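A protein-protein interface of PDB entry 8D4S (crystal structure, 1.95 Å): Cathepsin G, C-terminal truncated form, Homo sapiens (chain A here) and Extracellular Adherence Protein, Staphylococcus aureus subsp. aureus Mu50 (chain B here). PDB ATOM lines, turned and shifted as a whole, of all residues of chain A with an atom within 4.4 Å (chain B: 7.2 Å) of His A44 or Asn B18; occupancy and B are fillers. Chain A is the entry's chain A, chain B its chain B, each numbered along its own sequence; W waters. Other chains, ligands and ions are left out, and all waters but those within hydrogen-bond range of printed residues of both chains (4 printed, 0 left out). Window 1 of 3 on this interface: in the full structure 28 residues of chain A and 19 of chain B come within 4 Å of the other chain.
The backbone carbonyl oxygen (O) of Ser A196 is in hydrogen-bond range of the backbone NH (N) of Asn B18 (3.1 Å). The backbone NH of Ser B16 is in hydrogen-bond range of the backbone carbonyl oxygen of Gly A198 (2.8 Å). The side-chain hydroxyl (OG) of Ser A181 lies within hydrogen-bond range of the backbone NH (N) of Ile B19, at 3.2 Å. The backbone carbonyl oxygen (O) of Asn B18 lies close to the side-chain hydroxyl (OG) of Ser A181. The backbone carbonyl oxygen (O) of Asn B18 sits at hydrogen-bond distance from the backbone NH (N) of Gly A179. The backbone carbonyl oxygen of Asn B18 lies close to the backbone carbonyl oxygen of Phe A177, at 3.2 Å. The side-chain amino group (NZ) of Lys A178 is in hydrogen-bond range of the side-chain hydroxyl (OG) of Ser B16, at 2.6 Å. O of Asn B18 lies within hydrogen-bond range of N of Asp A180. The backbone NH (N) of Leu B20 lies close to the backbone NH (N) of Gly A179 (3.4 Å). NZ of Lys A178 lies within hydrogen-bond range of O of Gln B17 (2.9 Å). OE1 of Glu A206 is in hydrogen-bond range of ND2 of Asn B18, at 3.4 Å.
The side-chain carboxylate (OE2) of Glu A206 is in hydrogen-bond range of the backbone NH (N) of Ala A176, at 2.8 Å. A ring nitrogen (ND1) of His A44 sits at hydrogen-bond distance from the side-chain carboxylate (OD2) of Asp A88 (2.7 Å). The side-chain carboxylate (OD2) of Asp A88 is in hydrogen-bond range of the side-chain hydroxyl (OG) of Ser A196 (2.7 Å). OD2 of Asp A180 lies within hydrogen-bond range of N of Phe A177, 2.7 Å away. A ring nitrogen (NE2) of His A44 is in hydrogen-bond range of the side-chain hydroxyl (OG) of Ser A181 (2.6 Å). The side-chain hydroxyl (OG) of Ser A181 sits at hydrogen-bond distance from the backbone carbonyl oxygen (O) of Ser A196 (3.5 Å).
His A44 touches Ile B19. Trp A46 touches Phe B46. Gln B17 touches Tyr A80 (NE2 to OH, 3.9 Å). Lys A178 touches Ile B19. Lys A178 touches Leu B20. C of Ile B19 touches N of Gly A179, at 3.5 Å. Val A195 touches Asn B18. Ser A196 touches Gln B17 (O to CA, 3.8 Å). CB of Tyr A197 touches O of Ser B16, 3.4 Å away. C of Tyr A197 touches ND2 of Asn B18 (3.8 Å).
Of the printed residues of chain B, His A44 touches Gln B17 (3.3 Å), Asn B18 (3.99 Å) and Ile B19 (3.7 Å). Printed residues of chain B within 4 Å of Tyr A80: Gln B17. Printed residues of chain B within 4 Å of Ala A176: Asn B18. Of the printed residues of chain B, Phe A177 touches Asn B18 (3.2 Å). Printed residues of chain B within 4 Å of Ser A196: Gln B17 and Asn B18. Of the printed residues of chain A, Asn B18 touches His A44 (3.99 Å), Ala A176 (3.8 Å), Phe A177 (3.2 Å), Lys A178 (3.6 Å), Gly A179 (2.8 Å), Asp A180 (3.4 Å), Ser A181 (2.8 Å), Val A195 (3.6 Å), Ser A196 (3.1 Å), Tyr A197 (3.8 Å) and Glu A206 (3.4 Å). Ser B21 touches none of the printed residues of chain A. The nearest printed residue of chain B that does not touch Glu A206 is Ser B16 (7.6 Å).
Hydrophobic or aromatic side chains of chain B that line the printed part of chain A: Ile B19, Leu B20 and Phe B46. Along chain A the printed residues that touch a printed residue of chain B span positions 44 to 206. Among the printed residues, 25 pairs touch across the chains. Among the printed residues, no Asp or Glu carboxylate lies within 4 Å of a Lys or Arg side-chain nitrogen of the other chain.
Water W1 lies within hydrogen-bond range of NE2 of Gln B17 (2.6 Å) and OH of Tyr A80 (2.8 Å). Water W3 bridges OH of Tyr A80 (2.7 Å) and O of Asn B47 (3.0 Å). Water W2 lies within hydrogen-bond range of the backbone carbonyl oxygen (O) of Ala A176 (2.7 Å), the side-chain carboxylate (OE1) of Glu A206 (2.9 Å) and the side-chain amide nitrogen (ND2) of Asn B18 (3.4 Å). Water W4 lies within hydrogen-bond range of the side-chain carboxylate (OE1) of Glu A206 (2.9 Å), the side-chain amide nitrogen (ND2) of Asn B18 (2.9 Å), the backbone NH (N) of Ser A196 (3.1 Å) and the backbone carbonyl oxygen (O) of Tyr A197 (3.2 Å).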
ATOM      1  N   ALA A  42     -16.738   2.056   1.952  1.00  0.00           N
ATOM      2  CA  ALA A  42     -17.588   2.459   3.061  1.00  0.00           C
ATOM      3  C   ALA A  42     -17.888   1.272   3.962  1.00  0.00           C
ATOM      4  O   ALA A  42     -18.016   0.137   3.499  1.00  0.00           O
ATOM      5  CB  ALA A  42     -18.902   3.055   2.550  1.00  0.00           C
ATOM      6  N   ALA A  43     -18.029   1.554   5.259  1.00  0.00           N
ATOM      7  CA  ALA A  43     -18.385   0.502   6.203  1.00  0.00           C
ATOM      8  C   ALA A  43     -19.778  -0.063   5.944  1.00  0.00           C
ATOM      9  O   ALA A  43     -20.027  -1.236   6.247  1.00  0.00           O
ATOM     10  CB  ALA A  43     -18.291   1.020   7.640  1.00  0.00           C
ATOM     11  N   HIS A  44     -20.713   0.737   5.416  1.00  0.00           N
ATOM     12  CA  HIS A  44     -22.042   0.172   5.189  1.00  0.00           C
ATOM     13  C   HIS A  44     -22.079  -0.728   3.958  1.00  0.00           C
ATOM     14  O   HIS A  44     -23.124  -1.314   3.656  1.00  0.00           O
ATOM     15  CB  HIS A  44     -23.109   1.276   5.082  1.00  0.00           C
ATOM     16  CG  HIS A  44     -23.032   2.103   3.831  1.00  0.00           C
ATOM     17  ND1 HIS A  44     -22.375   3.315   3.770  1.00  0.00           N
ATOM     18  CD2 HIS A  44     -23.575   1.912   2.603  1.00  0.00           C
ATOM     19  CE1 HIS A  44     -22.482   3.816   2.552  1.00  0.00           C
ATOM     20  NE2 HIS A  44     -23.217   2.990   1.825  1.00  0.00           N
ATOM     21  N   CYS A  45     -20.971  -0.851   3.244  1.00  0.00           N
ATOM     22  CA  CYS A  45     -20.842  -1.867   2.209  1.00  0.00           C
ATOM     23  C   CYS A  45     -20.377  -3.220   2.747  1.00  0.00           C
ATOM     24  O   CYS A  45     -20.012  -4.092   1.956  1.00  0.00           O
ATOM     25  CB  CYS A  45     -19.875  -1.370   1.143  1.00  0.00           C
ATOM     26  SG  CYS A  45     -20.432   0.173   0.395  1.00  0.00           S
ATOM     27  N   TRP A  46     -20.379  -3.418   4.061  1.00  0.00           N
ATOM     28  CA  TRP A  46     -19.888  -4.663   4.636  1.00  0.00           C
ATOM     29  C   TRP A  46     -20.837  -5.825   4.343  1.00  0.00           C
ATOM     30  O   TRP A  46     -22.051  -5.651   4.209  1.00  0.00           O
ATOM     31  CB  TRP A  46     -19.717  -4.511   6.150  1.00  0.00           C
ATOM     32  CG  TRP A  46     -19.227  -5.752   6.853  1.00  0.00           C
ATOM     33  CD1 TRP A  46     -17.929  -6.093   7.086  1.00  0.00           C
ATOM     34  CD2 TRP A  46     -20.025  -6.805   7.419  1.00  0.00           C
ATOM     35  NE1 TRP A  46     -17.867  -7.287   7.759  1.00  0.00           N
ATOM     36  CE2 TRP A  46     -19.136  -7.747   7.976  1.00  0.00           C
ATOM     37  CE3 TRP A  46     -21.404  -7.039   7.520  1.00  0.00           C
ATOM     38  CZ2 TRP A  46     -19.576  -8.907   8.614  1.00  0.00           C
ATOM     39  CZ3 TRP A  46     -21.839  -8.194   8.157  1.00  0.00           C
ATOM     40  CH2 TRP A  46     -20.929  -9.110   8.695  1.00  0.00           C
ATOM     41  N   TYR A  80     -17.742   2.574  13.799  1.00  0.00           N
ATOM     42  CA  TYR A  80     -18.815   2.697  12.825  1.00  0.00           C
ATOM     43  C   TYR A  80     -20.172   2.657  13.523  1.00  0.00           C
ATOM     44  O   TYR A  80     -20.426   1.798  14.366  1.00  0.00           O
ATOM     45  CB  TYR A  80     -18.704   1.573  11.797  1.00  0.00           C
ATOM     46  CG  TYR A  80     -19.880   1.491  10.860  1.00  0.00           C
ATOM     47  CD1 TYR A  80     -20.283   2.601  10.130  1.00  0.00           C
ATOM     48  CD2 TYR A  80     -20.577   0.304  10.699  1.00  0.00           C
ATOM     49  CE1 TYR A  80     -21.357   2.536   9.276  1.00  0.00           C
ATOM     50  CE2 TYR A  80     -21.648   0.219   9.825  1.00  0.00           C
ATOM     51  CZ  TYR A  80     -22.039   1.335   9.135  1.00  0.00           C
ATOM     52  OH  TYR A  80     -23.100   1.267   8.286  1.00  0.00           O
ATOM     53  N   ASP A  88     -17.835   6.030   8.711  1.00  0.00           N
ATOM     54  CA  ASP A  88     -18.278   5.105   7.664  1.00  0.00           C
ATOM     55  C   ASP A  88     -17.096   4.765   6.755  1.00  0.00           C
ATOM     56  O   ASP A  88     -16.956   5.272   5.648  1.00  0.00           O
ATOM     57  CB  ASP A  88     -19.427   5.729   6.879  1.00  0.00           C
ATOM     58  CG  ASP A  88     -20.106   4.739   5.922  1.00  0.00           C
ATOM     59  OD1 ASP A  88     -19.903   3.514   6.055  1.00  0.00           O
ATOM     60  OD2 ASP A  88     -20.847   5.196   5.033  1.00  0.00           O
ATOM     61  N   ALA A 176     -23.134  11.820  -6.466  1.00  0.00           N
ATOM     62  CA  ALA A 176     -23.009  10.372  -6.421  1.00  0.00           C
ATOM     63  C   ALA A 176     -24.335   9.803  -5.935  1.00  0.00           C
ATOM     64  O   ALA A 176     -25.085  10.473  -5.216  1.00  0.00           O
ATOM     65  CB  ALA A 176     -21.857   9.963  -5.504  1.00  0.00           C
ATOM     66  N   PHE A 177     -24.659   8.584  -6.355  1.00  0.00           N
ATOM     67  CA  PHE A 177     -26.011   8.073  -6.101  1.00  0.00           C
ATOM     68  C   PHE A 177     -25.935   6.583  -5.764  1.00  0.00           C
ATOM     69  O   PHE A 177     -24.895   6.075  -5.322  1.00  0.00           O
ATOM     70  CB  PHE A 177     -26.918   8.416  -7.292  1.00  0.00           C
ATOM     71  CG  PHE A 177     -28.387   8.382  -6.967  1.00  0.00           C
ATOM     72  CD1 PHE A 177     -28.861   8.914  -5.770  1.00  0.00           C
ATOM     73  CD2 PHE A 177     -29.293   7.819  -7.857  1.00  0.00           C
ATOM     74  CE1 PHE A 177     -30.220   8.885  -5.468  1.00  0.00           C
ATOM     75  CE2 PHE A 177     -30.651   7.777  -7.562  1.00  0.00           C
ATOM     76  CZ  PHE A 177     -31.115   8.316  -6.367  1.00  0.00           C
ATOM     77  N   LYS A 178     -27.054   5.873  -5.938  1.00  0.00           N
ATOM     78  CA  LYS A 178     -27.190   4.513  -5.414  1.00  0.00           C
ATOM     79  C   LYS A 178     -26.275   3.565  -6.174  1.00  0.00           C
ATOM     80  O   LYS A 178     -26.424   3.402  -7.382  1.00  0.00           O
ATOM     81  CB  LYS A 178     -28.644   4.045  -5.520  1.00  0.00           C
ATOM     82  CG  LYS A 178     -29.658   4.996  -4.844  1.00  0.00           C
ATOM     83  CD  LYS A 178     -29.272   5.275  -3.399  1.00  0.00           C
ATOM     84  CE  LYS A 178     -30.382   6.034  -2.639  1.00  0.00           C
ATOM     85  NZ  LYS A 178     -29.861   6.547  -1.332  1.00  0.00           N
ATOM     86  N   GLY A 179     -25.328   2.934  -5.472  1.00  0.00           N
ATOM     87  CA  GLY A 179     -24.292   2.160  -6.124  1.00  0.00           C
ATOM     88  C   GLY A 179     -22.919   2.804  -6.104  1.00  0.00           C
ATOM     89  O   GLY A 179     -21.930   2.108  -6.354  1.00  0.00           O
ATOM     90  N   ASP A 180     -22.817   4.100  -5.812  1.00  0.00           N
ATOM     91  CA  ASP A 180     -21.528   4.787  -5.780  1.00  0.00           C
ATOM     92  C   ASP A 180     -20.879   4.815  -4.395  1.00  0.00           C
ATOM     93  O   ASP A 180     -19.729   5.237  -4.297  1.00  0.00           O
ATOM     94  CB  ASP A 180     -21.685   6.218  -6.287  1.00  0.00           C
ATOM     95  CG  ASP A 180     -22.197   6.269  -7.706  1.00  0.00           C
ATOM     96  OD1 ASP A 180     -21.708   5.474  -8.540  1.00  0.00           O
ATOM     97  OD2 ASP A 180     -23.095   7.096  -7.977  1.00  0.00           O
ATOM     98  N   SER A 181     -21.599   4.409  -3.334  1.00  0.00           N
ATOM     99  CA  SER A 181     -21.016   4.249  -1.997  1.00  0.00           C
ATOM    100  C   SER A 181     -19.662   3.564  -2.053  1.00  0.00           C
ATOM    101  O   SER A 181     -19.477   2.590  -2.777  1.00  0.00           O
ATOM    102  CB  SER A 181     -21.926   3.397  -1.120  1.00  0.00           C
ATOM    103  OG  SER A 181     -22.905   4.155  -0.465  1.00  0.00           O
ATOM    104  N   VAL A 195     -17.513   8.069  -0.885  1.00  0.00           N
ATOM    105  CA  VAL A 195     -18.948   8.311  -0.991  1.00  0.00           C
ATOM    106  C   VAL A 195     -19.653   7.626   0.165  1.00  0.00           C
ATOM    107  O   VAL A 195     -19.405   6.445   0.446  1.00  0.00           O
ATOM    108  CB  VAL A 195     -19.489   7.812  -2.338  1.00  0.00           C
ATOM    109  CG1 VAL A 195     -21.004   8.063  -2.428  1.00  0.00           C
ATOM    110  CG2 VAL A 195     -18.744   8.473  -3.482  1.00  0.00           C
ATOM    111  N   SER A 196     -20.524   8.365   0.856  1.00  0.00           N
ATOM    112  CA  SER A 196     -21.196   7.763   1.996  1.00  0.00           C
ATOM    113  C   SER A 196     -22.719   7.876   1.909  1.00  0.00           C
ATOM    114  O   SER A 196     -23.392   6.868   1.660  1.00  0.00           O
ATOM    115  CB  SER A 196     -20.665   8.377   3.298  1.00  0.00           C
ATOM    116  OG  SER A 196     -21.320   7.799   4.422  1.00  0.00           O
ATOM    117  N   TYR A 197     -23.299   9.055   2.122  1.00  0.00           N
ATOM    118  CA  TYR A 197     -24.755   9.100   2.124  1.00  0.00           C
ATOM    119  C   TYR A 197     -25.263  10.432   1.592  1.00  0.00           C
ATOM    120  O   TYR A 197     -24.499  11.373   1.383  1.00  0.00           O
ATOM    121  CB  TYR A 197     -25.308   8.810   3.523  1.00  0.00           C
ATOM    122  CG  TYR A 197     -25.023   9.836   4.605  1.00  0.00           C
ATOM    123  CD1 TYR A 197     -25.870  10.921   4.798  1.00  0.00           C
ATOM    124  CD2 TYR A 197     -23.943   9.691   5.475  1.00  0.00           C
ATOM    125  CE1 TYR A 197     -25.633  11.855   5.805  1.00  0.00           C
ATOM    126  CE2 TYR A 197     -23.709  10.616   6.486  1.00  0.00           C
ATOM    127  CZ  TYR A 197     -24.565  11.688   6.646  1.00  0.00           C
ATOM    128  OH  TYR A 197     -24.347  12.604   7.643  1.00  0.00           O
ATOM    129  N   GLY A 198     -26.569  10.486   1.355  1.00  0.00           N
ATOM    130  CA  GLY A 198     -27.228  11.722   0.971  1.00  0.00           C
ATOM    131  C   GLY A 198     -28.722  11.687   1.245  1.00  0.00           C
ATOM    132  O   GLY A 198     -29.206  10.983   2.140  1.00  0.00           O
ATOM    133  N   GLU A 206     -24.251  16.220  -0.419  1.00  0.00           N
ATOM    134  CA  GLU A 206     -24.149  14.876   0.115  1.00  0.00           C
ATOM    135  C   GLU A 206     -22.897  14.784   0.972  1.00  0.00           C
ATOM    136  O   GLU A 206     -22.019  15.645   0.915  1.00  0.00           O
ATOM    137  CB  GLU A 206     -24.103  13.849  -1.005  1.00  0.00           C
ATOM    138  CG  GLU A 206     -22.976  14.095  -1.957  1.00  0.00           C
ATOM    139  CD  GLU A 206     -22.991  13.108  -3.122  1.00  0.00           C
ATOM    140  OE1 GLU A 206     -23.377  11.937  -2.911  1.00  0.00           O
ATOM    141  OE2 GLU A 206     -22.628  13.513  -4.245  1.00  0.00           O
ATOM    142  N   SER B  16     -29.763   8.638   3.658  1.00  0.00           N
ATOM    143  CA  SER B  16     -29.922   7.415   2.881  1.00  0.00           C
ATOM    144  C   SER B  16     -28.564   7.020   2.337  1.00  0.00           C
ATOM    145  O   SER B  16     -27.918   7.824   1.660  1.00  0.00           O
ATOM    146  CB  SER B  16     -30.926   7.630   1.741  1.00  0.00           C
ATOM    147  OG  SER B  16     -31.085   6.466   0.962  1.00  0.00           O
ATOM    148  N   GLN B  17     -28.130   5.793   2.633  1.00  0.00           N
ATOM    149  CA  GLN B  17     -26.833   5.327   2.153  1.00  0.00           C
ATOM    150  C   GLN B  17     -26.851   5.235   0.636  1.00  0.00           C
ATOM    151  O   GLN B  17     -27.875   4.903   0.027  1.00  0.00           O
ATOM    152  CB  GLN B  17     -26.487   3.954   2.747  1.00  0.00           C
ATOM    153  CG  GLN B  17     -26.467   3.857   4.277  1.00  0.00           C
ATOM    154  CD  GLN B  17     -26.507   2.409   4.750  1.00  0.00           C
ATOM    155  OE1 GLN B  17     -26.867   1.509   3.988  1.00  0.00           O
ATOM    156  NE2 GLN B  17     -26.110   2.174   5.989  1.00  0.00           N
ATOM    157  N   ASN B  18     -25.716   5.519   0.022  1.00  0.00           N
ATOM    158  CA  ASN B  18     -25.629   5.456  -1.435  1.00  0.00           C
ATOM    159  C   ASN B  18     -25.296   4.069  -1.960  1.00  0.00           C
ATOM    160  O   ASN B  18     -24.582   3.936  -2.947  1.00  0.00           O
ATOM    161  CB  ASN B  18     -24.618   6.483  -1.932  1.00  0.00           C
ATOM    162  CG  ASN B  18     -25.244   7.860  -2.064  1.00  0.00           C
ATOM    163  OD1 ASN B  18     -26.430   7.974  -2.402  1.00  0.00           O
ATOM    164  ND2 ASN B  18     -24.471   8.903  -1.794  1.00  0.00           N
ATOM    165  N   ILE B  19     -25.804   3.040  -1.319  1.00  0.00           N
ATOM    166  CA  ILE B  19     -25.596   1.660  -1.722  1.00  0.00           C
ATOM    167  C   ILE B  19     -26.687   1.304  -2.720  1.00  0.00           C
ATOM    168  O   ILE B  19     -27.769   1.898  -2.712  1.00  0.00           O
ATOM    169  CB  ILE B  19     -25.621   0.746  -0.482  1.00  0.00           C
ATOM    170  CG1 ILE B  19     -25.216  -0.682  -0.834  1.00  0.00           C
ATOM    171  CG2 ILE B  19     -27.007   0.789   0.184  1.00  0.00           C
ATOM    172  CD1 ILE B  19     -24.797  -1.484   0.367  1.00  0.00           C
ATOM    173  N   LEU B  20     -26.402   0.360  -3.610  1.00  0.00           N
ATOM    174  CA  LEU B  20     -27.415  -0.193  -4.505  1.00  0.00           C
ATOM    175  C   LEU B  20     -27.774  -1.564  -3.951  1.00  0.00           C
ATOM    176  O   LEU B  20     -26.972  -2.502  -4.021  1.00  0.00           O
ATOM    177  CB  LEU B  20     -26.896  -0.279  -5.933  1.00  0.00           C
ATOM    178  CG  LEU B  20     -27.921  -0.842  -6.923  1.00  0.00           C
ATOM    179  CD1 LEU B  20     -29.189   0.025  -6.926  1.00  0.00           C
ATOM    180  CD2 LEU B  20     -27.321  -0.887  -8.296  1.00  0.00           C
ATOM    181  N   SER B  21     -28.953  -1.680  -3.369  1.00  0.00           N
ATOM    182  CA  SER B  21     -29.290  -2.860  -2.590  1.00  0.00           C
ATOM    183  C   SER B  21     -30.587  -3.470  -3.091  1.00  0.00           C
ATOM    184  O   SER B  21     -31.529  -2.752  -3.429  1.00  0.00           O
ATOM    185  CB  SER B  21     -29.399  -2.512  -1.112  1.00  0.00           C
ATOM    186  OG  SER B  21     -30.119  -1.307  -0.955  1.00  0.00           O
ATOM    187  N   PHE B  46     -30.169  -5.077   9.066  1.00  0.00           N
ATOM    188  CA  PHE B  46     -28.826  -5.281   8.531  1.00  0.00           C
ATOM    189  C   PHE B  46     -28.166  -3.958   8.167  1.00  0.00           C
ATOM    190  O   PHE B  46     -26.985  -3.749   8.461  1.00  0.00           O
ATOM    191  CB  PHE B  46     -28.872  -6.204   7.307  1.00  0.00           C
ATOM    192  CG  PHE B  46     -27.505  -6.588   6.776  1.00  0.00           C
ATOM    193  CD1 PHE B  46     -26.711  -7.505   7.456  1.00  0.00           C
ATOM    194  CD2 PHE B  46     -27.021  -6.035   5.601  1.00  0.00           C
ATOM    195  CE1 PHE B  46     -25.456  -7.864   6.971  1.00  0.00           C
ATOM    196  CE2 PHE B  46     -25.764  -6.387   5.111  1.00  0.00           C
ATOM    197  CZ  PHE B  46     -24.983  -7.305   5.797  1.00  0.00           C
ATOM    198  N   ASN B  47     -28.904  -3.055   7.519  1.00  0.00           N
ATOM    199  CA  ASN B  47     -28.293  -1.849   6.962  1.00  0.00           C
ATOM    200  C   ASN B  47     -28.203  -0.699   7.960  1.00  0.00           C
ATOM    201  O   ASN B  47     -27.220   0.047   7.957  1.00  0.00           O
ATOM    202  CB  ASN B  47     -29.080  -1.380   5.741  1.00  0.00           C
ATOM    203  CG  ASN B  47     -28.862  -2.263   4.548  1.00  0.00           C
ATOM    204  OD1 ASN B  47     -27.728  -2.568   4.173  1.00  0.00           O
ATOM    205  ND2 ASN B  47     -29.948  -2.688   3.943  1.00  0.00           N
ATOM    206  N   ARG B  48     -29.226  -0.508   8.793  1.00  0.00           N
ATOM    207  CA  ARG B  48     -29.234   0.657   9.666  1.00  0.00           C
ATOM    208  C   ARG B  48     -29.437   0.293  11.129  1.00  0.00           C
ATOM    209  O   ARG B  48     -29.672   1.188  11.948  1.00  0.00           O
ATOM    210  CB  ARG B  48     -30.299   1.667   9.210  1.00  0.00           C
ATOM    211  CG  ARG B  48     -30.056   2.257   7.815  1.00  0.00           C
ATOM    212  CD  ARG B  48     -28.762   3.090   7.722  1.00  0.00           C
ATOM    213  NE  ARG B  48     -28.856   4.355   8.461  1.00  0.00           N
ATOM    214  CZ  ARG B  48     -29.334   5.486   7.943  1.00  0.00           C
ATOM    215  NH1 ARG B  48     -29.784   5.517   6.698  1.00  0.00           N
ATOM    216  NH2 ARG B  48     -29.387   6.577   8.680  1.00  0.00           N
HETATM  217  O   HOH W   1     -25.027   3.252   8.032  1.00  0.00           O
HETATM  218  O   HOH W   2     -26.268  11.575  -3.015  1.00  0.00           O
HETATM  219  O   HOH W   3     -24.460  -1.082   8.081  1.00  0.00           O
HETATM  220  O   HOH W   4     -22.230  10.455  -0.700  1.00  0.00           O
